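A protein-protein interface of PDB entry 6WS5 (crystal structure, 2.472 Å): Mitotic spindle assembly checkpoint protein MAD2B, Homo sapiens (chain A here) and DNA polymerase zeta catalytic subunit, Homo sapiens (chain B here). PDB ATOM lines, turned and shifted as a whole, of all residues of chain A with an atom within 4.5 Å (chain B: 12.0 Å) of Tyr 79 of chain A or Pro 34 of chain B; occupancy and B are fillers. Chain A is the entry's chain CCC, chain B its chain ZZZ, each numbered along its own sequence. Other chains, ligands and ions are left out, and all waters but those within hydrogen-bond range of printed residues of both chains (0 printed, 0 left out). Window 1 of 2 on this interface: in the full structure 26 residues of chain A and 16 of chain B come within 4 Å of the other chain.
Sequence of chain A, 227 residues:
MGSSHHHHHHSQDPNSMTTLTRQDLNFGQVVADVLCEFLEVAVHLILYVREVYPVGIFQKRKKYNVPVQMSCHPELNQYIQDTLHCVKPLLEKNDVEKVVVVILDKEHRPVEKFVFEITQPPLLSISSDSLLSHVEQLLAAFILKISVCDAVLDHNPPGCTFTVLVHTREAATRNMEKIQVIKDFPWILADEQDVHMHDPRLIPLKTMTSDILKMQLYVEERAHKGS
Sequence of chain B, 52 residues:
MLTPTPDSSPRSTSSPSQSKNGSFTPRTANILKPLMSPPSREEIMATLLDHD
Of the 14 printed residues of chain B, 9 touch a printed residue of chain A. Along chain B the printed residues that touch a printed residue of chain A span positions 32 to 43. Printed residues of chain A that touch a printed residue of chain B: Glu 75, Leu 76, Tyr 79, Phe 162, Val 164, Phe 185, Pro 186 and Trp 187. Hydrophobic or aromatic side chains of chain A that line the printed part of chain B: Tyr 79, Phe 162, Phe 185, Pro 186 and Trp 187. Among the printed residues, 17 pairs touch across the chains.
The backbone carbonyl oxygen of Met 36 of chain B is in hydrogen-bond range of the side-chain hydroxyl of Tyr 79 of chain A (2.7 Å). The backbone carbonyl oxygen (O) of Pro 186 of chain A is in hydrogen-bond range of the backbone NH (N) of Leu 35 of chain B (3.1 Å). The side-chain carboxylate (OE2) of Glu 75 of chain A sits close to the side-chain carboxylate (OE1) of Glu 43 of chain B, 2.9 Å away.
Leu 76 of chain A touches Pro 39 of chain B (N to CG, 3.7 Å). Tyr 79 of chain A touches Pro 34 of chain B (OH to CB, 3.5 Å). Tyr 79 of chain A touches Pro 38 of chain B. Phe 162 of chain A touches Pro 38 of chain B. Val 164 of chain A touches Leu 32 of chain B. Val 164 of chain A touches Lys 33 of chain B (O to CA, 3.8 Å). Phe 185 of chain A touches Pro 34 of chain B. Trp 187 of chain A touches Leu 32 of chain B (CZ3 to C, 3.9 Å). CE3 of Trp 187 of chain A touches C of Lys 33 of chain B, at 3.2 Å. N of Pro 34 of chain B touches CE3 of Trp 187 of chain A (3.4 Å).
OG1 of Thr 83 of chain A lies within hydrogen-bond range of O of Tyr 79 of chain A (2.9 Å). N of Glu 43 of chain B lies within hydrogen-bond range of OG of Ser 40 of chain B (3.3 Å).
Tyr 79 of chain A touches just these residues of chain B: Pro 34, Met 36, Ser 37 and Pro 38. No residue of chain B comes within 4 Å of Asp 82 of chain A. No residue of chain B comes within 4 Å of Thr 83 of chain A. Of chain B, only Leu 32 (3.9 Å), Lys 33 (3.8 Å) and Pro 34 (3.1 Å) come within 4 Å of Val 164 of chain A. Of the printed residues of chain A, Leu 32 of chain B touches Val 164 (3.9 Å) and Trp 187 (3.9 Å). Pro 34 of chain B touches five residues of chain A. Printed residues of chain A within 4 Å of Pro 38 of chain B: Tyr 79 and Phe 162. Of the printed residues of chain A, Pro 39 of chain B touches Glu 75 (3.6 Å) and Leu 76 (3.7 Å). Ser 40 of chain B touches none of the printed residues of chain A. Printed residues of chain A within 4 Å of Glu 43 of chain B: Glu 75. The nearest residue of chain B that does not touch Tyr 79 of chain A is Pro 39 of chain B (4.2 Å). The nearest printed residue of chain A that does not touch Leu 35 of chain B is Trp 187 of chain A (4.4 Å).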
ATOM      1  N   GLU A  75       8.362  12.684  17.678  1.00  0.00           N
ATOM      2  CA  GLU A  75       7.717  11.672  18.536  1.00  0.00           C
ATOM      3  C   GLU A  75       6.866  12.359  19.610  1.00  0.00           C
ATOM      4  O   GLU A  75       5.650  12.051  19.682  1.00  0.00           O
ATOM      5  CB  GLU A  75       8.803  10.807  19.159  1.00  0.00           C
ATOM      6  CG  GLU A  75       8.271   9.658  19.993  1.00  0.00           C
ATOM      7  CD  GLU A  75       9.325   8.622  20.394  1.00  0.00           C
ATOM      8  OE1 GLU A  75       8.977   7.687  21.154  1.00  0.00           O
ATOM      9  OE2 GLU A  75      10.495   8.737  19.928  1.00  0.00           O
ATOM     10  N   LEU A  76       7.441  13.283  20.393  1.00  0.00           N
ATOM     11  CA  LEU A  76       6.656  14.093  21.347  1.00  0.00           C
ATOM     12  C   LEU A  76       5.482  14.705  20.597  1.00  0.00           C
ATOM     13  O   LEU A  76       4.345  14.593  21.154  1.00  0.00           O
ATOM     14  CB  LEU A  76       7.482  15.201  22.031  1.00  0.00           C
ATOM     15  CG  LEU A  76       6.673  16.105  22.975  1.00  0.00           C
ATOM     16  CD1 LEU A  76       5.937  15.267  24.046  1.00  0.00           C
ATOM     17  CD2 LEU A  76       7.558  17.114  23.682  1.00  0.00           C
ATOM     18  N   ASN A  77       5.728  15.332  19.424  1.00  0.00           N
ATOM     19  CA  ASN A  77       4.676  16.080  18.642  1.00  0.00           C
ATOM     20  C   ASN A  77       3.559  15.087  18.248  1.00  0.00           C
ATOM     21  O   ASN A  77       2.374  15.398  18.368  1.00  0.00           O
ATOM     22  CB  ASN A  77       5.267  16.829  17.443  1.00  0.00           C
ATOM     23  CG  ASN A  77       6.305  17.908  17.788  1.00  0.00           C
ATOM     24  OD1 ASN A  77       6.600  18.218  18.958  1.00  0.00           O
ATOM     25  ND2 ASN A  77       6.902  18.511  16.764  1.00  0.00           N
ATOM     26  N   GLN A  78       3.947  13.855  17.904  1.00  0.00           N
ATOM     27  CA  GLN A  78       3.028  12.796  17.467  1.00  0.00           C
ATOM     28  C   GLN A  78       2.185  12.360  18.675  1.00  0.00           C
ATOM     29  O   GLN A  78       0.902  12.280  18.589  1.00  0.00           O
ATOM     30  CB  GLN A  78       3.840  11.638  16.894  1.00  0.00           C
ATOM     31  CG  GLN A  78       2.971  10.534  16.325  1.00  0.00           C
ATOM     32  CD  GLN A  78       2.302  11.072  15.091  1.00  0.00           C
ATOM     33  OE1 GLN A  78       2.987  11.489  14.140  1.00  0.00           O
ATOM     34  NE2 GLN A  78       0.973  11.131  15.133  1.00  0.00           N
ATOM     35  N   TYR A  79       2.860  12.084  19.808  1.00  0.00           N
ATOM     36  CA  TYR A  79       2.084  11.648  20.996  1.00  0.00           C
ATOM     37  C   TYR A  79       0.948  12.650  21.285  1.00  0.00           C
ATOM     38  O   TYR A  79      -0.170  12.203  21.531  1.00  0.00           O
ATOM     39  CB  TYR A  79       2.997  11.475  22.188  1.00  0.00           C
ATOM     40  CG  TYR A  79       2.238  11.006  23.402  1.00  0.00           C
ATOM     41  CD1 TYR A  79       2.268   9.660  23.731  1.00  0.00           C
ATOM     42  CD2 TYR A  79       1.622  11.901  24.281  1.00  0.00           C
ATOM     43  CE1 TYR A  79       1.706   9.194  24.918  1.00  0.00           C
ATOM     44  CE2 TYR A  79       1.020  11.447  25.459  1.00  0.00           C
ATOM     45  CZ  TYR A  79       1.084  10.087  25.777  1.00  0.00           C
ATOM     46  OH  TYR A  79       0.513   9.590  26.878  1.00  0.00           O
ATOM     47  N   ILE A  80       1.225  13.972  21.222  1.00  0.00           N
ATOM     48  CA  ILE A  80       0.287  15.058  21.582  1.00  0.00           C
ATOM     49  C   ILE A  80      -0.813  15.118  20.515  1.00  0.00           C
ATOM     50  O   ILE A  80      -1.996  15.283  20.888  1.00  0.00           O
ATOM     51  CB  ILE A  80       1.019  16.401  21.709  1.00  0.00           C
ATOM     52  CG1 ILE A  80       1.820  16.493  23.007  1.00  0.00           C
ATOM     53  CG2 ILE A  80       0.019  17.530  21.604  1.00  0.00           C
ATOM     54  CD1 ILE A  80       3.037  17.414  22.904  1.00  0.00           C
ATOM     55  N   GLN A  81      -0.415  14.976  19.262  1.00  0.00           N
ATOM     56  CA  GLN A  81      -1.292  15.007  18.046  1.00  0.00           C
ATOM     57  C   GLN A  81      -2.306  13.861  18.074  1.00  0.00           C
ATOM     58  O   GLN A  81      -3.537  14.194  18.120  1.00  0.00           O
ATOM     59  CB  GLN A  81      -0.433  14.935  16.793  1.00  0.00           C
ATOM     60  CG  GLN A  81      -1.232  15.048  15.511  1.00  0.00           C
ATOM     61  CD  GLN A  81      -0.462  15.793  14.451  1.00  0.00           C
ATOM     62  OE1 GLN A  81      -0.371  15.352  13.310  1.00  0.00           O
ATOM     63  NE2 GLN A  81       0.106  16.916  14.864  1.00  0.00           N
ATOM     64  N   ASP A  82      -1.800  12.646  18.249  1.00  0.00           N
ATOM     65  CA  ASP A  82      -2.546  11.353  18.476  1.00  0.00           C
ATOM     66  C   ASP A  82      -3.484  11.460  19.669  1.00  0.00           C
ATOM     67  O   ASP A  82      -4.685  11.071  19.521  1.00  0.00           O
ATOM     68  CB  ASP A  82      -1.677  10.132  18.842  1.00  0.00           C
ATOM     69  CG  ASP A  82      -0.759   9.610  17.736  1.00  0.00           C
ATOM     70  OD1 ASP A  82      -1.026   9.928  16.538  1.00  0.00           O
ATOM     71  OD2 ASP A  82       0.268   8.938  18.089  1.00  0.00           O
ATOM     72  N   THR A  83      -2.978  11.992  20.794  1.00  0.00           N
ATOM     73  CA  THR A  83      -3.836  12.276  21.973  1.00  0.00           C
ATOM     74  C   THR A  83      -5.050  13.086  21.488  1.00  0.00           C
ATOM     75  O   THR A  83      -6.203  12.681  21.770  1.00  0.00           O
ATOM     76  CB  THR A  83      -3.100  12.934  23.150  1.00  0.00           C
ATOM     77  OG1 THR A  83      -2.118  12.032  23.659  1.00  0.00           O
ATOM     78  CG2 THR A  83      -4.044  13.194  24.311  1.00  0.00           C
ATOM     79  N   PHE A 162       4.752  13.666  32.152  1.00  0.00           N
ATOM     80  CA  PHE A 162       3.354  14.146  32.051  1.00  0.00           C
ATOM     81  C   PHE A 162       2.497  13.057  31.390  1.00  0.00           C
ATOM     82  O   PHE A 162       3.019  12.281  30.602  1.00  0.00           O
ATOM     83  CB  PHE A 162       3.277  15.406  31.199  1.00  0.00           C
ATOM     84  CG  PHE A 162       3.146  15.177  29.707  1.00  0.00           C
ATOM     85  CD1 PHE A 162       4.251  14.932  28.933  1.00  0.00           C
ATOM     86  CD2 PHE A 162       1.922  15.278  29.063  1.00  0.00           C
ATOM     87  CE1 PHE A 162       4.147  14.798  27.552  1.00  0.00           C
ATOM     88  CE2 PHE A 162       1.801  15.180  27.668  1.00  0.00           C
ATOM     89  CZ  PHE A 162       2.904  14.891  26.910  1.00  0.00           C
ATOM     90  N   VAL A 164      -1.961  12.670  29.949  1.00  0.00           N
ATOM     91  CA  VAL A 164      -3.277  13.334  29.697  1.00  0.00           C
ATOM     92  C   VAL A 164      -4.485  12.539  30.221  1.00  0.00           C
ATOM     93  O   VAL A 164      -4.727  11.497  29.721  1.00  0.00           O
ATOM     94  CB  VAL A 164      -3.432  13.560  28.199  1.00  0.00           C
ATOM     95  CG1 VAL A 164      -4.832  14.168  27.889  1.00  0.00           C
ATOM     96  CG2 VAL A 164      -2.299  14.425  27.677  1.00  0.00           C
ATOM     97  N   PHE A 185      -2.335   3.258  19.517  1.00  0.00           N
ATOM     98  CA  PHE A 185      -2.615   4.311  20.520  1.00  0.00           C
ATOM     99  C   PHE A 185      -3.915   4.044  21.267  1.00  0.00           C
ATOM    100  O   PHE A 185      -4.741   4.913  21.384  1.00  0.00           O
ATOM    101  CB  PHE A 185      -2.672   5.725  19.936  1.00  0.00           C
ATOM    102  CG  PHE A 185      -2.358   6.801  20.953  1.00  0.00           C
ATOM    103  CD1 PHE A 185      -1.048   7.070  21.305  1.00  0.00           C
ATOM    104  CD2 PHE A 185      -3.378   7.553  21.536  1.00  0.00           C
ATOM    105  CE1 PHE A 185      -0.765   8.081  22.238  1.00  0.00           C
ATOM    106  CE2 PHE A 185      -3.104   8.556  22.455  1.00  0.00           C
ATOM    107  CZ  PHE A 185      -1.776   8.808  22.834  1.00  0.00           C
ATOM    108  N   PRO A 186      -4.066   2.913  21.984  1.00  0.00           N
ATOM    109  CA  PRO A 186      -5.291   2.688  22.741  1.00  0.00           C
ATOM    110  C   PRO A 186      -5.392   3.474  24.055  1.00  0.00           C
ATOM    111  O   PRO A 186      -4.437   4.030  24.563  1.00  0.00           O
ATOM    112  CB  PRO A 186      -5.164   1.197  23.032  1.00  0.00           C
ATOM    113  CG  PRO A 186      -3.675   1.051  23.283  1.00  0.00           C
ATOM    114  CD  PRO A 186      -3.052   1.874  22.184  1.00  0.00           C
ATOM    115  N   TRP A 187      -6.596   3.457  24.585  1.00  0.00           N
ATOM    116  CA  TRP A 187      -7.032   4.221  25.765  1.00  0.00           C
ATOM    117  C   TRP A 187      -7.511   3.254  26.840  1.00  0.00           C
ATOM    118  O   TRP A 187      -7.958   2.156  26.474  1.00  0.00           O
ATOM    119  CB  TRP A 187      -8.101   5.203  25.302  1.00  0.00           C
ATOM    120  CG  TRP A 187      -7.585   6.418  24.565  1.00  0.00           C
ATOM    121  CD1 TRP A 187      -7.225   6.522  23.234  1.00  0.00           C
ATOM    122  CD2 TRP A 187      -7.326   7.703  25.136  1.00  0.00           C
ATOM    123  NE1 TRP A 187      -6.801   7.784  22.945  1.00  0.00           N
ATOM    124  CE2 TRP A 187      -6.846   8.528  24.102  1.00  0.00           C
ATOM    125  CE3 TRP A 187      -7.521   8.235  26.415  1.00  0.00           C
ATOM    126  CZ2 TRP A 187      -6.522   9.872  24.323  1.00  0.00           C
ATOM    127  CZ3 TRP A 187      -7.285   9.572  26.618  1.00  0.00           C
ATOM    128  CH2 TRP A 187      -6.760  10.362  25.594  1.00  0.00           C
ATOM    129  N   ASN B  30     -15.553   7.453  34.411  1.00  0.00           N
ATOM    130  CA  ASN B  30     -15.638   8.619  33.473  1.00  0.00           C
ATOM    131  C   ASN B  30     -14.272   9.261  33.186  1.00  0.00           C
ATOM    132  O   ASN B  30     -14.266  10.317  32.550  1.00  0.00           O
ATOM    133  CB  ASN B  30     -16.522   9.720  34.048  1.00  0.00           C
ATOM    134  CG  ASN B  30     -15.846  10.434  35.196  1.00  0.00           C
ATOM    135  OD1 ASN B  30     -15.485   9.821  36.204  1.00  0.00           O
ATOM    136  ND2 ASN B  30     -15.665  11.738  35.052  1.00  0.00           N
ATOM    137  N   ILE B  31     -13.163   8.675  33.666  1.00  0.00           N
ATOM    138  CA  ILE B  31     -11.761   9.156  33.447  1.00  0.00           C
ATOM    139  C   ILE B  31     -10.977   8.210  32.512  1.00  0.00           C
ATOM    140  O   ILE B  31     -10.719   6.962  32.892  1.00  0.00           O
ATOM    141  CB  ILE B  31     -11.095   9.405  34.796  1.00  0.00           C
ATOM    142  CG1 ILE B  31     -11.730  10.621  35.469  1.00  0.00           C
ATOM    143  CG2 ILE B  31      -9.593   9.584  34.632  1.00  0.00           C
ATOM    144  CD1 ILE B  31     -11.448  10.779  36.914  1.00  0.00           C
ATOM    145  N   LEU B  32     -10.603   8.758  31.331  1.00  0.00           N
ATOM    146  CA  LEU B  32      -9.850   8.036  30.278  1.00  0.00           C
ATOM    147  C   LEU B  32      -8.419   8.583  30.170  1.00  0.00           C
ATOM    148  O   LEU B  32      -8.147   9.763  30.491  1.00  0.00           O
ATOM    149  CB  LEU B  32     -10.597   8.167  28.946  1.00  0.00           C
ATOM    150  CG  LEU B  32     -11.929   7.438  28.861  1.00  0.00           C
ATOM    151  CD1 LEU B  32     -12.598   7.715  27.529  1.00  0.00           C
ATOM    152  CD2 LEU B  32     -11.724   5.957  29.072  1.00  0.00           C
ATOM    153  N   LYS B  33      -7.537   7.775  29.619  1.00  0.00           N
ATOM    154  CA  LYS B  33      -6.061   7.935  29.733  1.00  0.00           C
ATOM    155  C   LYS B  33      -5.444   7.119  28.615  1.00  0.00           C
ATOM    156  O   LYS B  33      -5.870   6.009  28.370  1.00  0.00           O
ATOM    157  CB  LYS B  33      -5.620   7.402  31.115  1.00  0.00           C
ATOM    158  CG  LYS B  33      -4.160   7.587  31.475  1.00  0.00           C
ATOM    159  CD  LYS B  33      -3.564   6.415  32.179  1.00  0.00           C
ATOM    160  CE  LYS B  33      -2.121   6.614  32.613  1.00  0.00           C
ATOM    161  NZ  LYS B  33      -1.162   6.858  31.486  1.00  0.00           N
ATOM    162  N   PRO B  34      -4.458   7.661  27.885  1.00  0.00           N
ATOM    163  CA  PRO B  34      -3.617   6.850  26.987  1.00  0.00           C
ATOM    164  C   PRO B  34      -2.901   5.730  27.771  1.00  0.00           C
ATOM    165  O   PRO B  34      -2.572   5.913  28.919  1.00  0.00           O
ATOM    166  CB  PRO B  34      -2.540   7.838  26.521  1.00  0.00           C
ATOM    167  CG  PRO B  34      -3.337   9.151  26.573  1.00  0.00           C
ATOM    168  CD  PRO B  34      -4.063   9.079  27.891  1.00  0.00           C
ATOM    169  N   LEU B  35      -2.895   4.536  27.221  1.00  0.00           N
ATOM    170  CA  LEU B  35      -2.159   3.402  27.776  1.00  0.00           C
ATOM    171  C   LEU B  35      -0.682   3.732  27.646  1.00  0.00           C
ATOM    172  O   LEU B  35       0.030   3.500  28.566  1.00  0.00           O
ATOM    173  CB  LEU B  35      -2.534   2.158  26.959  1.00  0.00           C
ATOM    174  CG  LEU B  35      -1.640   0.932  27.168  1.00  0.00           C
ATOM    175  CD1 LEU B  35      -1.809   0.452  28.613  1.00  0.00           C
ATOM    176  CD2 LEU B  35      -1.947  -0.158  26.151  1.00  0.00           C
ATOM    177  N   MET B  36      -0.268   4.271  26.506  1.00  0.00           N
ATOM    178  CA  MET B  36       1.131   4.697  26.174  1.00  0.00           C
ATOM    179  C   MET B  36       1.494   6.014  26.893  1.00  0.00           C
ATOM    180  O   MET B  36       0.657   6.919  27.072  1.00  0.00           O
ATOM    181  CB  MET B  36       1.270   4.949  24.677  1.00  0.00           C
ATOM    182  CG  MET B  36       0.930   3.733  23.803  1.00  0.00           C
ATOM    183  SD  MET B  36       1.863   2.235  24.233  1.00  0.00           S
ATOM    184  CE  MET B  36       1.333   1.172  22.882  1.00  0.00           C
ATOM    185  N   SER B  37       2.721   6.092  27.331  1.00  0.00           N
ATOM    186  CA  SER B  37       3.333   7.302  27.904  1.00  0.00           C
ATOM    187  C   SER B  37       3.982   8.126  26.792  1.00  0.00           C
ATOM    188  O   SER B  37       4.293   7.615  25.706  1.00  0.00           O
ATOM    189  CB  SER B  37       4.262   6.899  28.945  1.00  0.00           C
ATOM    190  OG  SER B  37       3.501   6.380  30.039  1.00  0.00           O
ATOM    191  N   PRO B  38       4.063   9.469  26.967  1.00  0.00           N
ATOM    192  CA  PRO B  38       4.849  10.289  26.061  1.00  0.00           C
ATOM    193  C   PRO B  38       6.278   9.775  26.168  1.00  0.00           C
ATOM    194  O   PRO B  38       6.695   9.260  27.221  1.00  0.00           O
ATOM    195  CB  PRO B  38       4.798  11.710  26.677  1.00  0.00           C
ATOM    196  CG  PRO B  38       3.977  11.652  27.935  1.00  0.00           C
ATOM    197  CD  PRO B  38       3.572  10.204  28.136  1.00  0.00           C
ATOM    198  N   PRO B  39       7.098   9.922  25.135  1.00  0.00           N
ATOM    199  CA  PRO B  39       8.536   9.714  25.279  1.00  0.00           C
ATOM    200  C   PRO B  39       9.101  10.391  26.530  1.00  0.00           C
ATOM    201  O   PRO B  39       8.663  11.508  26.761  1.00  0.00           O
ATOM    202  CB  PRO B  39       9.110  10.474  24.055  1.00  0.00           C
ATOM    203  CG  PRO B  39       7.912  11.085  23.308  1.00  0.00           C
ATOM    204  CD  PRO B  39       6.683  10.338  23.790  1.00  0.00           C
ATOM    205  N   SER B  40       9.956   9.715  27.328  1.00  0.00           N
ATOM    206  CA  SER B  40      10.590  10.251  28.578  1.00  0.00           C
ATOM    207  C   SER B  40      11.623  11.367  28.286  1.00  0.00           C
ATOM    208  O   SER B  40      11.976  11.584  27.078  1.00  0.00           O
ATOM    209  CB  SER B  40      11.266   9.169  29.319  1.00  0.00           C
ATOM    210  OG  SER B  40      12.343   8.616  28.574  1.00  0.00           O
ATOM    211  N   ARG B  41      12.069  12.080  29.318  1.00  0.00           N
ATOM    212  CA  ARG B  41      13.160  13.116  29.219  1.00  0.00           C
ATOM    213  C   ARG B  41      14.429  12.464  28.672  1.00  0.00           C
ATOM    214  O   ARG B  41      15.096  13.104  27.869  1.00  0.00           O
ATOM    215  CB  ARG B  41      13.541  13.759  30.565  1.00  0.00           C
ATOM    216  CG  ARG B  41      12.812  15.050  30.882  1.00  0.00           C
ATOM    217  CD  ARG B  41      13.467  15.899  31.955  1.00  0.00           C
ATOM    218  NE  ARG B  41      14.570  16.658  31.378  1.00  0.00           N
ATOM    219  CZ  ARG B  41      14.599  17.983  31.127  1.00  0.00           C
ATOM    220  NH1 ARG B  41      13.576  18.789  31.392  1.00  0.00           N
ATOM    221  NH2 ARG B  41      15.689  18.505  30.586  1.00  0.00           N
ATOM    222  N   GLU B  43      14.770   9.553  26.610  1.00  0.00           N
ATOM    223  CA  GLU B  43      14.570   9.200  25.178  1.00  0.00           C
ATOM    224  C   GLU B  43      14.826  10.434  24.300  1.00  0.00           C
ATOM    225  O   GLU B  43      15.354  10.300  23.182  1.00  0.00           O
ATOM    226  CB  GLU B  43      13.149   8.636  24.988  1.00  0.00           C
ATOM    227  CG  GLU B  43      12.999   7.598  23.874  1.00  0.00           C
ATOM    228  CD  GLU B  43      12.560   8.101  22.500  1.00  0.00           C
ATOM    229  OE1 GLU B  43      12.432   7.251  21.575  1.00  0.00           O
ATOM    230  OE2 GLU B  43      12.353   9.339  22.336  1.00  0.00           O
ATOM    231  N   ILE B  44      14.459  11.612  24.798  1.00  0.00           N
ATOM    232  CA  ILE B  44      14.623  12.929  24.113  1.00  0.00           C
ATOM    233  C   ILE B  44      16.072  13.398  24.269  1.00  0.00           C
ATOM    234  O   ILE B  44      16.690  13.624  23.244  1.00  0.00           O
ATOM    235  CB  ILE B  44      13.611  13.933  24.701  1.00  0.00           C
ATOM    236  CG1 ILE B  44      12.174  13.428  24.543  1.00  0.00           C
ATOM    237  CG2 ILE B  44      13.805  15.317  24.132  1.00  0.00           C
ATOM    238  CD1 ILE B  44      11.700  13.420  23.145  1.00  0.00           C
